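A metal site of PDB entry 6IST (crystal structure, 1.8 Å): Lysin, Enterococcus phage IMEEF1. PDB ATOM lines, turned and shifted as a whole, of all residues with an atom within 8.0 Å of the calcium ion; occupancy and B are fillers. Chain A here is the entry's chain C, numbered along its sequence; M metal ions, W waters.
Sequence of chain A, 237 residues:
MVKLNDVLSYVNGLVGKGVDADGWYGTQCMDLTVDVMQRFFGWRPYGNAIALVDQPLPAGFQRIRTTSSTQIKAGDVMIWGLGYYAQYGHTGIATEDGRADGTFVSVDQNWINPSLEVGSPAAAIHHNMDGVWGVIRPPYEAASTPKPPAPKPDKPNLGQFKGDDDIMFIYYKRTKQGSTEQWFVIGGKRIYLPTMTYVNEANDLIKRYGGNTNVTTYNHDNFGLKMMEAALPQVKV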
ATOM      1  N   VAL A  19      21.036  14.949 -15.497  1.00  0.00           N
ATOM      2  CA  VAL A  19      20.931  14.776 -16.909  1.00  0.00           C
ATOM      3  C   VAL A  19      19.558  14.331 -17.265  1.00  0.00           C
ATOM      4  O   VAL A  19      18.949  13.568 -16.532  1.00  0.00           O
ATOM      5  CB  VAL A  19      21.972  13.819 -17.501  1.00  0.00           C
ATOM      6  CG1 VAL A  19      23.302  14.563 -17.515  1.00  0.00           C
ATOM      7  CG2 VAL A  19      22.083  12.508 -16.780  1.00  0.00           C
ATOM      8  N   ASP A  20      19.053  14.847 -18.396  1.00  0.00           N
ATOM      9  CA  ASP A  20      17.725  14.522 -18.904  1.00  0.00           C
ATOM     10  C   ASP A  20      17.958  13.927 -20.276  1.00  0.00           C
ATOM     11  O   ASP A  20      18.295  14.650 -21.188  1.00  0.00           O
ATOM     12  CB  ASP A  20      16.837  15.801 -19.022  1.00  0.00           C
ATOM     13  CG  ASP A  20      15.397  15.495 -19.516  1.00  0.00           C
ATOM     14  OD1 ASP A  20      15.055  14.286 -19.744  1.00  0.00           O
ATOM     15  OD2 ASP A  20      14.580  16.435 -19.662  1.00  0.00           O
ATOM     16  N   ALA A  21      17.806  12.623 -20.423  1.00  0.00           N
ATOM     17  CA  ALA A  21      18.132  11.933 -21.673  1.00  0.00           C
ATOM     18  C   ALA A  21      16.972  11.870 -22.629  1.00  0.00           C
ATOM     19  O   ALA A  21      17.180  11.710 -23.818  1.00  0.00           O
ATOM     20  CB  ALA A  21      18.625  10.519 -21.385  1.00  0.00           C
ATOM     21  N   ASP A  22      15.773  12.034 -22.136  1.00  0.00           N
ATOM     22  CA  ASP A  22      14.631  11.770 -22.951  1.00  0.00           C
ATOM     23  C   ASP A  22      13.690  12.914 -23.139  1.00  0.00           C
ATOM     24  O   ASP A  22      12.796  12.778 -23.960  1.00  0.00           O
ATOM     25  CB  ASP A  22      13.917  10.563 -22.419  1.00  0.00           C
ATOM     26  CG  ASP A  22      13.255  10.778 -21.087  1.00  0.00           C
ATOM     27  OD1 ASP A  22      13.417  11.865 -20.424  1.00  0.00           O
ATOM     28  OD2 ASP A  22      12.516   9.835 -20.680  1.00  0.00           O
ATOM     29  N   GLY A  23      13.881  14.038 -22.450  1.00  0.00           N
ATOM     30  CA  GLY A  23      12.952  15.167 -22.602  1.00  0.00           C
ATOM     31  C   GLY A  23      11.630  15.007 -21.920  1.00  0.00           C
ATOM     32  O   GLY A  23      10.713  15.736 -22.281  1.00  0.00           O
ATOM     33  N   TRP A  24      11.508  14.103 -20.939  1.00  0.00           N
ATOM     34  CA  TRP A  24      10.306  13.924 -20.123  1.00  0.00           C
ATOM     35  C   TRP A  24      10.640  13.939 -18.655  1.00  0.00           C
ATOM     36  O   TRP A  24      11.568  13.262 -18.267  1.00  0.00           O
ATOM     37  CB  TRP A  24       9.709  12.579 -20.376  1.00  0.00           C
ATOM     38  CG  TRP A  24       9.074  12.458 -21.674  1.00  0.00           C
ATOM     39  CD1 TRP A  24       9.660  12.126 -22.858  1.00  0.00           C
ATOM     40  CD2 TRP A  24       7.668  12.627 -21.945  1.00  0.00           C
ATOM     41  NE1 TRP A  24       8.710  12.139 -23.873  1.00  0.00           N
ATOM     42  CE2 TRP A  24       7.483  12.404 -23.330  1.00  0.00           C
ATOM     43  CE3 TRP A  24       6.564  12.972 -21.155  1.00  0.00           C
ATOM     44  CZ2 TRP A  24       6.247  12.512 -23.947  1.00  0.00           C
ATOM     45  CZ3 TRP A  24       5.303  13.039 -21.770  1.00  0.00           C
ATOM     46  CH2 TRP A  24       5.171  12.821 -23.166  1.00  0.00           C
ATOM     47  N   TYR A  25       9.877  14.698 -17.891  1.00  0.00           N
ATOM     48  CA  TYR A  25       9.854  14.678 -16.440  1.00  0.00           C
ATOM     49  C   TYR A  25      11.189  15.009 -15.777  1.00  0.00           C
ATOM     50  O   TYR A  25      11.516  14.471 -14.695  1.00  0.00           O
ATOM     51  CB  TYR A  25       9.347  13.380 -15.926  1.00  0.00           C
ATOM     52  CG  TYR A  25       7.997  13.009 -16.453  1.00  0.00           C
ATOM     53  CD1 TYR A  25       6.891  13.843 -16.245  1.00  0.00           C
ATOM     54  CD2 TYR A  25       7.830  11.814 -17.151  1.00  0.00           C
ATOM     55  CE1 TYR A  25       5.632  13.492 -16.753  1.00  0.00           C
ATOM     56  CE2 TYR A  25       6.578  11.459 -17.644  1.00  0.00           C
ATOM     57  CZ  TYR A  25       5.490  12.288 -17.419  1.00  0.00           C
ATOM     58  OH  TYR A  25       4.271  11.891 -17.892  1.00  0.00           O
ATOM     59  N   GLY A  26      12.120  15.895 -16.410  1.00  0.00           N
ATOM     60  CA  GLY A  26      13.485  16.305 -16.019  1.00  0.00           C
ATOM     61  C   GLY A  26      14.403  15.127 -15.760  1.00  0.00           C
ATOM     62  O   GLY A  26      14.572  14.217 -16.604  1.00  0.00           O
ATOM     63  N   THR A  27      15.022  15.112 -14.577  1.00  0.00           N
ATOM     64  CA  THR A  27      16.158  14.209 -14.369  1.00  0.00           C
ATOM     65  C   THR A  27      15.722  13.003 -13.534  1.00  0.00           C
ATOM     66  O   THR A  27      15.873  12.966 -12.362  1.00  0.00           O
ATOM     67  CB  THR A  27      17.319  15.015 -13.781  1.00  0.00           C
ATOM     68  OG1 THR A  27      16.937  15.513 -12.488  1.00  0.00           O
ATOM     69  CG2 THR A  27      17.692  16.188 -14.757  1.00  0.00           C
ATOM     70  N   GLN A  28      15.059  12.026 -14.169  1.00  0.00           N
ATOM     71  CA  GLN A  28      14.624  10.815 -13.538  1.00  0.00           C
ATOM     72  C   GLN A  28      15.754   9.796 -13.360  1.00  0.00           C
ATOM     73  O   GLN A  28      16.857  10.004 -13.911  1.00  0.00           O
ATOM     74  CB  GLN A  28      13.519  10.215 -14.349  1.00  0.00           C
ATOM     75  CG  GLN A  28      12.298  11.160 -14.447  1.00  0.00           C
ATOM     76  CD  GLN A  28      11.529  11.281 -13.144  1.00  0.00           C
ATOM     77  OE1 GLN A  28      11.307  10.297 -12.421  1.00  0.00           O
ATOM     78  NE2 GLN A  28      11.086  12.487 -12.834  1.00  0.00           N
ATOM     79  N   CYS A  29      15.475   8.721 -12.664  1.00  0.00           N
ATOM     80  CA  CYS A  29      16.535   7.703 -12.431  1.00  0.00           C
ATOM     81  C   CYS A  29      17.061   7.059 -13.697  1.00  0.00           C
ATOM     82  O   CYS A  29      18.306   6.955 -13.923  1.00  0.00           O
ATOM     83  CB  CYS A  29      16.134   6.725 -11.410  1.00  0.00           C
ATOM     84  SG  CYS A  29      14.901   5.495 -11.942  1.00  0.00           S
ATOM     85  N   MET A  30      16.132   6.678 -14.583  1.00  0.00           N
ATOM     86  CA  MET A  30      16.574   6.042 -15.825  1.00  0.00           C
ATOM     87  C   MET A  30      17.398   6.960 -16.733  1.00  0.00           C
ATOM     88  O   MET A  30      18.252   6.485 -17.503  1.00  0.00           O
ATOM     89  CB  MET A  30      15.320   5.446 -16.530  1.00  0.00           C
ATOM     90  CG  MET A  30      15.491   4.337 -17.577  1.00  0.00           C
ATOM     91  SD  MET A  30      16.645   2.984 -17.324  1.00  0.00           S
ATOM     92  CE  MET A  30      16.120   1.821 -18.647  1.00  0.00           C
ATOM     93  N   ASP A  31      17.142   8.286 -16.697  1.00  0.00           N
ATOM     94  CA  ASP A  31      17.921   9.237 -17.424  1.00  0.00           C
ATOM     95  C   ASP A  31      19.417   9.098 -17.190  1.00  0.00           C
ATOM     96  O   ASP A  31      20.164   9.258 -18.104  1.00  0.00           O
ATOM     97  CB  ASP A  31      17.497  10.673 -17.149  1.00  0.00           C
ATOM     98  CG  ASP A  31      16.152  11.013 -17.765  1.00  0.00           C
ATOM     99  OD1 ASP A  31      16.026  10.988 -19.002  1.00  0.00           O
ATOM    100  OD2 ASP A  31      15.231  11.320 -16.994  1.00  0.00           O
ATOM    101  N   LEU A  32      19.841   8.861 -15.943  1.00  0.00           N
ATOM    102  CA  LEU A  32      21.251   8.737 -15.677  1.00  0.00           C
ATOM    103  C   LEU A  32      21.832   7.489 -16.314  1.00  0.00           C
ATOM    104  O   LEU A  32      22.868   7.539 -16.993  1.00  0.00           O
ATOM    105  CB  LEU A  32      21.493   8.625 -14.154  1.00  0.00           C
ATOM    106  CG  LEU A  32      22.971   8.444 -13.770  1.00  0.00           C
ATOM    107  CD1 LEU A  32      23.730   9.601 -14.362  1.00  0.00           C
ATOM    108  CD2 LEU A  32      23.086   8.474 -12.258  1.00  0.00           C
ATOM    109  N   GLN A 109      19.881   9.374  -9.748  1.00  0.00           N
ATOM    110  CA  GLN A 109      18.955  10.509  -9.782  1.00  0.00           C
ATOM    111  C   GLN A 109      17.656  10.145  -9.249  1.00  0.00           C
ATOM    112  O   GLN A 109      17.238   8.989  -9.349  1.00  0.00           O
ATOM    113  CB  GLN A 109      18.773  11.038 -11.212  1.00  0.00           C
ATOM    114  CG  GLN A 109      20.034  11.634 -11.738  1.00  0.00           C
ATOM    115  CD  GLN A 109      19.972  12.237 -13.112  1.00  0.00           C
ATOM    116  OE1 GLN A 109      20.828  13.054 -13.435  1.00  0.00           O
ATOM    117  NE2 GLN A 109      19.031  11.799 -13.960  1.00  0.00           N
ATOM    118  N   GLU A 117       7.594  15.233 -11.321  1.00  0.00           N
ATOM    119  CA  GLU A 117       7.502  16.218 -12.376  1.00  0.00           C
ATOM    120  C   GLU A 117       8.880  16.564 -12.964  1.00  0.00           C
ATOM    121  O   GLU A 117       9.004  16.703 -14.134  1.00  0.00           O
ATOM    122  CB  GLU A 117       6.885  17.546 -11.848  1.00  0.00           C
ATOM    123  CG  GLU A 117       5.529  17.410 -11.123  1.00  0.00           C
ATOM    124  CD  GLU A 117       5.610  16.793  -9.690  1.00  0.00           C
ATOM    125  OE1 GLU A 117       4.548  16.394  -9.137  1.00  0.00           O
ATOM    126  OE2 GLU A 117       6.711  16.702  -9.108  1.00  0.00           O
ATOM    127  N   VAL A 118       9.885  16.751 -12.107  1.00  0.00           N
ATOM    128  CA  VAL A 118      11.204  17.247 -12.546  1.00  0.00           C
ATOM    129  C   VAL A 118      12.411  16.382 -12.115  1.00  0.00           C
ATOM    130  O   VAL A 118      13.512  16.672 -12.528  1.00  0.00           O
ATOM    131  CB  VAL A 118      11.408  18.713 -12.106  1.00  0.00           C
ATOM    132  CG1 VAL A 118      10.273  19.598 -12.667  1.00  0.00           C
ATOM    133  CG2 VAL A 118      11.486  18.870 -10.599  1.00  0.00           C
ATOM    134  N   GLY A 119      12.140  15.323 -11.392  1.00  0.00           N
ATOM    135  CA  GLY A 119      13.169  14.407 -10.892  1.00  0.00           C
ATOM    136  C   GLY A 119      14.048  15.265 -10.023  1.00  0.00           C
ATOM    137  O   GLY A 119      13.592  16.143  -9.315  1.00  0.00           O
HETATM  138 CA    CA M   1      13.816  12.886 -18.318  1.00  0.00          CA
HETATM  139  O   HOH W   1      11.802  10.496 -17.796  1.00  0.00           O
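OD1 of Asp 20 sits close to N of Gly 23, at 3.0 Å. N of Gln 28 lies close to OD2 of Asp 31, at 2.9 Å. OD1 of Asp 31 sits at hydrogen-bond distance from N of Ala 21 (2.8 Å).
Within 4 Å of the calcium ion: Asp 20, Asp 22, Trp 24, Gly 26 and Asp 31. The nearest printed residue that does not touch the calcium ion is Tyr 25 (4.2 Å).
The calcium ion is bound by the backbone carbonyl oxygen of Trp 24, the backbone carbonyl oxygen of Gly 26, the side-chain carboxylate of Asp 20, the side-chain carboxylate of Asp 22 and the side-chain carboxylate of Asp 31. The calcium ion has five donor atoms within binding distance. Slightly farther from the calcium ion lies OD1 of Asp 31 (3.0 Å).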
